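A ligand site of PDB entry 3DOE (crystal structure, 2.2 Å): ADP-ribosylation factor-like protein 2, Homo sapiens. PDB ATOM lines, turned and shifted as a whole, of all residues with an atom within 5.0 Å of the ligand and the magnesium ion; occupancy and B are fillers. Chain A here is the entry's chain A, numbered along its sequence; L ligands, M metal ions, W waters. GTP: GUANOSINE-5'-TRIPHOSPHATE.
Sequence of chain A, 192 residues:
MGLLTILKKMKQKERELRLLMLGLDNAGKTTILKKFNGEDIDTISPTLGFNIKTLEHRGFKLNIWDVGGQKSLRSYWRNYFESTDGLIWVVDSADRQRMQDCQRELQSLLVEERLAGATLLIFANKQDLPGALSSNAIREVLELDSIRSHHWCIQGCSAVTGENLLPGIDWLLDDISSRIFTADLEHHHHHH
N of Thr 30 lies within hydrogen-bond range of O1A of the ligand, at 3.4 Å. O2G of the ligand sits close to N of Thr 47 (2.6 Å). O1B of the ligand lies within hydrogen-bond range of N of Lys 29 (3.2 Å). An oxygen (O1B) of the ligand lies within salt-bridge range of the side-chain amino group (NZ) of Lys 29 (2.6 Å). OD1 of Asp 128 is in hydrogen-bond range of N1 of the ligand, at 2.7 Å. The backbone NH (N) of Thr 31 lies within hydrogen-bond range of an oxygen (O1A) of the ligand. OG1 of Thr 31 lies within hydrogen-bond range of O1A of the ligand. An oxygen (O3A) of the ligand is in hydrogen-bond range of the backbone NH (N) of Gly 28. N of Gly 69 is in hydrogen-bond range of O3G of the ligand. The backbone NH (N) of Ala 159 sits at hydrogen-bond distance from an oxygen (O6) of the ligand (3.1 Å). OD1 of Asn 125 lies close to N7 of the ligand. An oxygen (O3B) of the ligand is in hydrogen-bond range of the backbone NH (N) of Asn 26, at 3.1 Å. The backbone NH (N) of Ala 27 sits at hydrogen-bond distance from an oxygen (O1B) of the ligand. An oxygen (O6) of the ligand lies close to the backbone NH (N) of Lys 126, at 3.5 Å. An oxygen (O4') of the ligand is in hydrogen-bond range of the side-chain amino group (NZ) of Lys 126 (3.3 Å). The backbone NH (N) of Val 160 lies within hydrogen-bond range of an oxygen (O6) of the ligand, 3.4 Å away.
OG1 of Thr 30 sits close to OD1 of Asp 66. NZ of Lys 29 lies within hydrogen-bond range of O of Leu 24, 2.7 Å away. OG of Ser 158 sits at hydrogen-bond distance from OD1 of Asp 128 (2.8 Å). N of Asp 25 sits at hydrogen-bond distance from O of Gly 69. The side-chain amide oxygen (OD1) of Asn 125 sits close to the backbone carbonyl oxygen (O) of Ala 27, 3.0 Å away. SG of Cys 157 sits at hydrogen-bond distance from ND2 of Asn 125, at 3.3 Å. NZ of Lys 126 is in hydrogen-bond range of O of Asn 26 (2.7 Å). N of Lys 126 sits at hydrogen-bond distance from O of Cys 157, 3.0 Å away.
Leu 24 touches the ligand (O to O1B, 3.6 Å). Asp 25 touches the ligand. CG2 of Ile 44 touches O2A of the ligand (3.5 Å). C of Pro 46 touches O2G of the ligand, 3.5 Å away. Gly 68 touches the ligand (CA to O3G, 3.8 Å). Leu 129 touches the ligand. Ser 158 touches the ligand. Hydrophobic or aromatic side chains that line the ligand: Ala 27, Ile 44, Pro 46, Leu 129, Ala 159 and Val 160. Of the 27 residues printed, 20 come within 4 Å of the ligand.
Within 4 Å of the magnesium ion: Thr 30 and Thr 47.
The magnesium ion is bound by water W2 (2.1 Å), water W4 (2.2 Å), O2G of the ligand (2.2 Å), OG1 of Thr 30 (2.2 Å), OG1 of Thr 47 (2.3 Å) and O2B of the ligand (2.3 Å). The magnesium ion has six donor atoms within binding distance.
Water W2 lies within hydrogen-bond range of O of Ser 45 (2.8 Å) and O3B of the ligand (3.4 Å). Water W4 lies within hydrogen-bond range of the side-chain carboxylate of Asp 66 and an oxygen (O3G) of the ligand. Water W5 lies within hydrogen-bond range of O1G of the ligand, O of Thr 47, N of Gln 70 and N of Gly 69. Water W3 lies within hydrogen-bond range of O1G of the ligand and N of Asn 26.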
ATOM      1  N   GLY A  23     -16.932 -13.557  22.622  1.00  0.00           N
ATOM      2  CA  GLY A  23     -16.715 -14.640  21.686  1.00  0.00           C
ATOM      3  C   GLY A  23     -15.615 -14.272  20.716  1.00  0.00           C
ATOM      4  O   GLY A  23     -15.229 -13.100  20.621  1.00  0.00           O
ATOM      5  N   LEU A  24     -15.101 -15.271  20.012  1.00  0.00           N
ATOM      6  CA  LEU A  24     -14.070 -15.058  19.007  1.00  0.00           C
ATOM      7  C   LEU A  24     -14.537 -14.037  17.977  1.00  0.00           C
ATOM      8  O   LEU A  24     -15.739 -13.881  17.750  1.00  0.00           O
ATOM      9  CB  LEU A  24     -13.713 -16.376  18.323  1.00  0.00           C
ATOM     10  CG  LEU A  24     -12.442 -17.123  18.745  1.00  0.00           C
ATOM     11  CD1 LEU A  24     -12.216 -17.099  20.273  1.00  0.00           C
ATOM     12  CD2 LEU A  24     -12.474 -18.563  18.232  1.00  0.00           C
ATOM     13  N   ASP A  25     -13.577 -13.336  17.371  1.00  0.00           N
ATOM     14  CA  ASP A  25     -13.887 -12.410  16.291  1.00  0.00           C
ATOM     15  C   ASP A  25     -14.640 -13.171  15.208  1.00  0.00           C
ATOM     16  O   ASP A  25     -14.401 -14.369  15.003  1.00  0.00           O
ATOM     17  CB  ASP A  25     -12.611 -11.810  15.713  1.00  0.00           C
ATOM     18  CG  ASP A  25     -11.708 -12.844  15.067  1.00  0.00           C
ATOM     19  OD1 ASP A  25     -10.943 -13.516  15.792  1.00  0.00           O
ATOM     20  OD2 ASP A  25     -11.769 -13.003  13.821  1.00  0.00           O
ATOM     21  N   ASN A  26     -15.566 -12.495  14.533  1.00  0.00           N
ATOM     22  CA  ASN A  26     -16.300 -13.074  13.413  1.00  0.00           C
ATOM     23  C   ASN A  26     -17.396 -14.095  13.812  1.00  0.00           C
ATOM     24  O   ASN A  26     -17.972 -14.753  12.952  1.00  0.00           O
ATOM     25  CB  ASN A  26     -15.319 -13.695  12.401  1.00  0.00           C
ATOM     26  CG  ASN A  26     -15.938 -13.912  11.041  1.00  0.00           C
ATOM     27  OD1 ASN A  26     -16.407 -12.962  10.395  1.00  0.00           O
ATOM     28  ND2 ASN A  26     -15.923 -15.153  10.567  1.00  0.00           N
ATOM     29  N   ALA A  27     -17.681 -14.206  15.111  1.00  0.00           N
ATOM     30  CA  ALA A  27     -18.698 -15.138  15.593  1.00  0.00           C
ATOM     31  C   ALA A  27     -20.122 -14.662  15.313  1.00  0.00           C
ATOM     32  O   ALA A  27     -21.033 -15.479  15.162  1.00  0.00           O
ATOM     33  CB  ALA A  27     -18.509 -15.399  17.086  1.00  0.00           C
ATOM     34  N   GLY A  28     -20.294 -13.347  15.239  1.00  0.00           N
ATOM     35  CA  GLY A  28     -21.608 -12.771  14.968  1.00  0.00           C
ATOM     36  C   GLY A  28     -22.225 -12.097  16.184  1.00  0.00           C
ATOM     37  O   GLY A  28     -23.446 -12.005  16.276  1.00  0.00           O
ATOM     38  N   LYS A  29     -21.379 -11.634  17.104  1.00  0.00           N
ATOM     39  CA  LYS A  29     -21.855 -10.991  18.328  1.00  0.00           C
ATOM     40  C   LYS A  29     -22.659  -9.727  18.027  1.00  0.00           C
ATOM     41  O   LYS A  29     -23.797  -9.582  18.485  1.00  0.00           O
ATOM     42  CB  LYS A  29     -20.673 -10.626  19.236  1.00  0.00           C
ATOM     43  CG  LYS A  29     -19.920 -11.807  19.803  1.00  0.00           C
ATOM     44  CD  LYS A  29     -18.762 -11.350  20.678  1.00  0.00           C
ATOM     45  CE  LYS A  29     -17.608 -10.767  19.865  1.00  0.00           C
ATOM     46  NZ  LYS A  29     -16.960 -11.771  18.978  1.00  0.00           N
ATOM     47  N   THR A  30     -22.062  -8.833  17.251  1.00  0.00           N
ATOM     48  CA  THR A  30     -22.666  -7.552  16.891  1.00  0.00           C
ATOM     49  C   THR A  30     -23.879  -7.706  15.974  1.00  0.00           C
ATOM     50  O   THR A  30     -24.833  -6.928  16.071  1.00  0.00           O
ATOM     51  CB  THR A  30     -21.608  -6.616  16.240  1.00  0.00           C
ATOM     52  OG1 THR A  30     -20.580  -6.313  17.212  1.00  0.00           O
ATOM     53  CG2 THR A  30     -22.252  -5.310  15.751  1.00  0.00           C
ATOM     54  N   THR A  31     -23.852  -8.710  15.090  1.00  0.00           N
ATOM     55  CA  THR A  31     -25.025  -9.022  14.263  1.00  0.00           C
ATOM     56  C   THR A  31     -26.192  -9.429  15.164  1.00  0.00           C
ATOM     57  O   THR A  31     -27.325  -8.980  14.948  1.00  0.00           O
ATOM     58  CB  THR A  31     -24.720 -10.142  13.236  1.00  0.00           C
ATOM     59  OG1 THR A  31     -23.578  -9.770  12.450  1.00  0.00           O
ATOM     60  CG2 THR A  31     -25.909 -10.373  12.311  1.00  0.00           C
ATOM     61  N   ILE A  44     -22.247  -4.058   8.946  1.00  0.00           N
ATOM     62  CA  ILE A  44     -21.604  -4.317  10.227  1.00  0.00           C
ATOM     63  C   ILE A  44     -20.129  -4.605   9.994  1.00  0.00           C
ATOM     64  O   ILE A  44     -19.776  -5.399   9.111  1.00  0.00           O
ATOM     65  CB  ILE A  44     -22.281  -5.506  10.962  1.00  0.00           C
ATOM     66  CG1 ILE A  44     -23.589  -5.027  11.616  1.00  0.00           C
ATOM     67  CG2 ILE A  44     -21.353  -6.126  12.010  1.00  0.00           C
ATOM     68  CD1 ILE A  44     -24.426  -6.129  12.241  1.00  0.00           C
ATOM     69  N   SER A  45     -19.271  -3.941  10.764  1.00  0.00           N
ATOM     70  CA  SER A  45     -17.828  -4.122  10.651  1.00  0.00           C
ATOM     71  C   SER A  45     -17.293  -4.762  11.934  1.00  0.00           C
ATOM     72  O   SER A  45     -17.913  -4.615  12.989  1.00  0.00           O
ATOM     73  CB  SER A  45     -17.162  -2.761  10.406  1.00  0.00           C
ATOM     74  OG  SER A  45     -15.751  -2.824  10.535  1.00  0.00           O
ATOM     75  N   PRO A  46     -16.148  -5.479  11.847  1.00  0.00           N
ATOM     76  CA  PRO A  46     -15.571  -6.025  13.076  1.00  0.00           C
ATOM     77  C   PRO A  46     -15.337  -4.938  14.116  1.00  0.00           C
ATOM     78  O   PRO A  46     -14.893  -3.837  13.772  1.00  0.00           O
ATOM     79  CB  PRO A  46     -14.238  -6.633  12.613  1.00  0.00           C
ATOM     80  CG  PRO A  46     -13.987  -6.061  11.253  1.00  0.00           C
ATOM     81  CD  PRO A  46     -15.345  -5.848  10.669  1.00  0.00           C
ATOM     82  N   THR A  47     -15.650  -5.250  15.364  1.00  0.00           N
ATOM     83  CA  THR A  47     -15.574  -4.281  16.460  1.00  0.00           C
ATOM     84  C   THR A  47     -14.151  -4.176  17.001  1.00  0.00           C
ATOM     85  O   THR A  47     -13.538  -5.173  17.380  1.00  0.00           O
ATOM     86  CB  THR A  47     -16.544  -4.645  17.599  1.00  0.00           C
ATOM     87  OG1 THR A  47     -17.832  -4.941  17.050  1.00  0.00           O
ATOM     88  CG2 THR A  47     -16.673  -3.501  18.594  1.00  0.00           C
ATOM     89  N   ASN A  51     -19.771  -2.250  21.802  1.00  0.00           N
ATOM     90  CA  ASN A  51     -21.095  -1.684  21.579  1.00  0.00           C
ATOM     91  C   ASN A  51     -21.971  -1.862  22.803  1.00  0.00           C
ATOM     92  O   ASN A  51     -21.935  -2.918  23.446  1.00  0.00           O
ATOM     93  CB  ASN A  51     -21.748  -2.347  20.361  1.00  0.00           C
ATOM     94  CG  ASN A  51     -20.988  -2.109  19.077  1.00  0.00           C
ATOM     95  OD1 ASN A  51     -20.772  -0.960  18.670  1.00  0.00           O
ATOM     96  ND2 ASN A  51     -20.577  -3.188  18.417  1.00  0.00           N
ATOM     97  N   ASP A  66     -21.386  -5.503  23.977  1.00  0.00           N
ATOM     98  CA  ASP A  66     -20.801  -6.369  22.961  1.00  0.00           C
ATOM     99  C   ASP A  66     -19.356  -5.930  22.720  1.00  0.00           C
ATOM    100  O   ASP A  66     -19.119  -4.837  22.198  1.00  0.00           O
ATOM    101  CB  ASP A  66     -21.658  -6.310  21.697  1.00  0.00           C
ATOM    102  CG  ASP A  66     -20.882  -6.595  20.428  1.00  0.00           C
ATOM    103  OD1 ASP A  66     -20.091  -7.564  20.397  1.00  0.00           O
ATOM    104  OD2 ASP A  66     -21.074  -5.844  19.449  1.00  0.00           O
ATOM    105  N   VAL A  67     -18.397  -6.774  23.101  1.00  0.00           N
ATOM    106  CA  VAL A  67     -16.977  -6.430  23.016  1.00  0.00           C
ATOM    107  C   VAL A  67     -16.257  -7.185  21.898  1.00  0.00           C
ATOM    108  O   VAL A  67     -16.369  -8.412  21.788  1.00  0.00           O
ATOM    109  CB  VAL A  67     -16.227  -6.686  24.357  1.00  0.00           C
ATOM    110  CG1 VAL A  67     -14.862  -6.029  24.354  1.00  0.00           C
ATOM    111  CG2 VAL A  67     -17.048  -6.202  25.543  1.00  0.00           C
ATOM    112  N   GLY A  68     -15.511  -6.447  21.071  1.00  0.00           N
ATOM    113  CA  GLY A  68     -14.733  -7.017  19.977  1.00  0.00           C
ATOM    114  C   GLY A  68     -13.924  -8.234  20.400  1.00  0.00           C
ATOM    115  O   GLY A  68     -13.282  -8.223  21.447  1.00  0.00           O
ATOM    116  N   GLY A  69     -13.969  -9.268  19.563  1.00  0.00           N
ATOM    117  CA  GLY A  69     -13.306 -10.536  19.866  1.00  0.00           C
ATOM    118  C   GLY A  69     -12.001 -10.762  19.146  1.00  0.00           C
ATOM    119  O   GLY A  69     -11.407 -11.845  19.261  1.00  0.00           O
ATOM    120  N   GLN A  70     -11.541  -9.761  18.402  1.00  0.00           N
ATOM    121  CA  GLN A  70     -10.231  -9.823  17.749  1.00  0.00           C
ATOM    122  C   GLN A  70      -9.188 -10.161  18.804  1.00  0.00           C
ATOM    123  O   GLN A  70      -9.207  -9.613  19.904  1.00  0.00           O
ATOM    124  CB  GLN A  70      -9.899  -8.488  17.084  1.00  0.00           C
ATOM    125  CG  GLN A  70      -8.720  -8.543  16.133  1.00  0.00           C
ATOM    126  CD  GLN A  70      -8.390  -7.184  15.550  1.00  0.00           C
ATOM    127  OE1 GLN A  70      -9.276  -6.373  15.314  1.00  0.00           O
ATOM    128  NE2 GLN A  70      -7.105  -6.938  15.310  1.00  0.00           N
ATOM    129  N   ASN A 125     -23.987 -19.960  16.732  1.00  0.00           N
ATOM    130  CA  ASN A 125     -24.463 -19.138  15.623  1.00  0.00           C
ATOM    131  C   ASN A 125     -24.134 -19.728  14.250  1.00  0.00           C
ATOM    132  O   ASN A 125     -23.311 -20.640  14.144  1.00  0.00           O
ATOM    133  CB  ASN A 125     -23.852 -17.741  15.772  1.00  0.00           C
ATOM    134  CG  ASN A 125     -24.574 -16.689  14.953  1.00  0.00           C
ATOM    135  OD1 ASN A 125     -23.949 -15.771  14.428  1.00  0.00           O
ATOM    136  ND2 ASN A 125     -25.883 -16.823  14.841  1.00  0.00           N
ATOM    137  N   LYS A 126     -24.772 -19.197  13.208  1.00  0.00           N
ATOM    138  CA  LYS A 126     -24.503 -19.557  11.805  1.00  0.00           C
ATOM    139  C   LYS A 126     -24.928 -20.985  11.431  1.00  0.00           C
ATOM    140  O   LYS A 126     -24.288 -21.615  10.589  1.00  0.00           O
ATOM    141  CB  LYS A 126     -23.044 -19.310  11.416  1.00  0.00           C
ATOM    142  CG  LYS A 126     -22.513 -17.944  11.819  1.00  0.00           C
ATOM    143  CD  LYS A 126     -21.227 -17.595  11.099  1.00  0.00           C
ATOM    144  CE  LYS A 126     -20.650 -16.296  11.626  1.00  0.00           C
ATOM    145  NZ  LYS A 126     -19.388 -15.940  10.934  1.00  0.00           N
ATOM    146  N   ASP A 128     -27.227 -21.677   9.685  1.00  0.00           N
ATOM    147  CA  ASP A 128     -27.674 -21.556   8.301  1.00  0.00           C
ATOM    148  C   ASP A 128     -26.606 -22.025   7.325  1.00  0.00           C
ATOM    149  O   ASP A 128     -26.897 -22.239   6.144  1.00  0.00           O
ATOM    150  CB  ASP A 128     -28.080 -20.113   7.994  1.00  0.00           C
ATOM    151  CG  ASP A 128     -26.942 -19.122   8.240  1.00  0.00           C
ATOM    152  OD1 ASP A 128     -26.680 -18.798   9.413  1.00  0.00           O
ATOM    153  OD2 ASP A 128     -26.325 -18.670   7.254  1.00  0.00           O
ATOM    154  N   LEU A 129     -25.378 -22.169   7.807  1.00  0.00           N
ATOM    155  CA  LEU A 129     -24.274 -22.644   6.970  1.00  0.00           C
ATOM    156  C   LEU A 129     -24.188 -24.164   6.972  1.00  0.00           C
ATOM    157  O   LEU A 129     -24.228 -24.782   8.043  1.00  0.00           O
ATOM    158  CB  LEU A 129     -22.945 -22.026   7.417  1.00  0.00           C
ATOM    159  CG  LEU A 129     -22.749 -20.520   7.179  1.00  0.00           C
ATOM    160  CD1 LEU A 129     -21.533 -20.001   7.947  1.00  0.00           C
ATOM    161  CD2 LEU A 129     -22.622 -20.190   5.696  1.00  0.00           C
ATOM    162  N   CYS A 157     -28.431 -21.216  16.589  1.00  0.00           N
ATOM    163  CA  CYS A 157     -29.158 -20.109  15.985  1.00  0.00           C
ATOM    164  C   CYS A 157     -28.513 -19.603  14.701  1.00  0.00           C
ATOM    165  O   CYS A 157     -27.482 -20.118  14.253  1.00  0.00           O
ATOM    166  CB  CYS A 157     -29.255 -18.948  16.978  1.00  0.00           C
ATOM    167  SG  CYS A 157     -27.660 -18.165  17.342  1.00  0.00           S
ATOM    168  N   SER A 158     -29.147 -18.597  14.120  1.00  0.00           N
ATOM    169  CA  SER A 158     -28.675 -17.918  12.938  1.00  0.00           C
ATOM    170  C   SER A 158     -29.024 -16.444  13.085  1.00  0.00           C
ATOM    171  O   SER A 158     -30.158 -16.034  12.792  1.00  0.00           O
ATOM    172  CB  SER A 158     -29.338 -18.516  11.685  1.00  0.00           C
ATOM    173  OG  SER A 158     -29.062 -17.737  10.528  1.00  0.00           O
ATOM    174  N   ALA A 159     -28.073 -15.650  13.567  1.00  0.00           N
ATOM    175  CA  ALA A 159     -28.262 -14.213  13.773  1.00  0.00           C
ATOM    176  C   ALA A 159     -28.749 -13.517  12.517  1.00  0.00           C
ATOM    177  O   ALA A 159     -29.616 -12.646  12.577  1.00  0.00           O
ATOM    178  CB  ALA A 159     -26.975 -13.584  14.247  1.00  0.00           C
ATOM    179  N   VAL A 160     -28.202 -13.930  11.381  1.00  0.00           N
ATOM    180  CA  VAL A 160     -28.549 -13.373  10.075  1.00  0.00           C
ATOM    181  C   VAL A 160     -30.058 -13.400   9.788  1.00  0.00           C
ATOM    182  O   VAL A 160     -30.590 -12.465   9.191  1.00  0.00           O
ATOM    183  CB  VAL A 160     -27.733 -14.054   8.932  1.00  0.00           C
ATOM    184  CG1 VAL A 160     -28.536 -14.214   7.650  1.00  0.00           C
ATOM    185  CG2 VAL A 160     -26.454 -13.269   8.667  1.00  0.00           C
HETATM  186  PG  GTP L   1     -16.072  -8.963  16.081  1.00  0.00           P
HETATM  187  O1G GTP L   1     -14.684  -9.026  15.499  1.00  0.00           O
HETATM  188  O2G GTP L   1     -16.557  -7.538  16.138  1.00  0.00           O
HETATM  189  O3G GTP L   1     -16.057  -9.549  17.470  1.00  0.00           O
HETATM  190  O3B GTP L   1     -17.070  -9.805  15.144  1.00  0.00           O
HETATM  191  PB  GTP L   1     -18.483 -10.351  15.718  1.00  0.00           P
HETATM  192  O1B GTP L   1     -18.233 -11.466  16.702  1.00  0.00           O
HETATM  193  O2B GTP L   1     -19.317  -9.233  16.318  1.00  0.00           O
HETATM  194  O3A GTP L   1     -19.174 -10.957  14.411  1.00  0.00           O
HETATM  195  PA  GTP L   1     -20.024 -10.053  13.396  1.00  0.00           P
HETATM  196  O1A GTP L   1     -21.369  -9.713  14.013  1.00  0.00           O
HETATM  197  O2A GTP L   1     -19.261  -8.807  12.999  1.00  0.00           O
HETATM  198  O5' GTP L   1     -20.217 -11.043  12.150  1.00  0.00           O
HETATM  199  C5' GTP L   1     -19.108 -11.370  11.320  1.00  0.00           C
HETATM  200  C4' GTP L   1     -19.597 -11.811   9.940  1.00  0.00           C
HETATM  201  O4' GTP L   1     -20.411 -12.967  10.071  1.00  0.00           O
HETATM  202  C3' GTP L   1     -20.462 -10.735   9.291  1.00  0.00           C
HETATM  203  O3' GTP L   1     -20.256 -10.721   7.884  1.00  0.00           O
HETATM  204  C2' GTP L   1     -21.880 -11.201   9.596  1.00  0.00           C
HETATM  205  O2' GTP L   1     -22.796 -10.719   8.651  1.00  0.00           O
HETATM  206  C1' GTP L   1     -21.694 -12.710   9.536  1.00  0.00           C
HETATM  207  N9  GTP L   1     -22.737 -13.433  10.282  1.00  0.00           N
HETATM  208  C8  GTP L   1     -23.222 -13.134  11.529  1.00  0.00           C
HETATM  209  N7  GTP L   1     -24.168 -14.049  11.855  1.00  0.00           N
HETATM  210  C5  GTP L   1     -24.281 -14.919  10.834  1.00  0.00           C
HETATM  211  C6  GTP L   1     -25.095 -16.031  10.628  1.00  0.00           C
HETATM  212  O6  GTP L   1     -25.887 -16.381  11.499  1.00  0.00           O
HETATM  213  N1  GTP L   1     -24.990 -16.743   9.448  1.00  0.00           N
HETATM  214  C2  GTP L   1     -24.097 -16.354   8.470  1.00  0.00           C
HETATM  215  N2  GTP L   1     -23.997 -17.039   7.336  1.00  0.00           N
HETATM  216  N3  GTP L   1     -23.296 -15.248   8.674  1.00  0.00           N
HETATM  217  C4  GTP L   1     -23.388 -14.540   9.833  1.00  0.00           C
HETATM  218 MG    MG M   1     -18.662  -6.997  16.402  1.00  0.00          MG
HETATM  219  O   HOH W   1     -19.791 -13.204   6.552  1.00  0.00           O
HETATM  220  O   HOH W   2     -18.686  -6.909  14.298  1.00  0.00           O
HETATM  221  O   HOH W   3     -14.701 -10.025  13.049  1.00  0.00           O
HETATM  222  O   HOH W   4     -18.273  -7.451  18.494  1.00  0.00           O
HETATM  223  O   HOH W   5     -12.964  -7.725  16.642  1.00  0.00           O
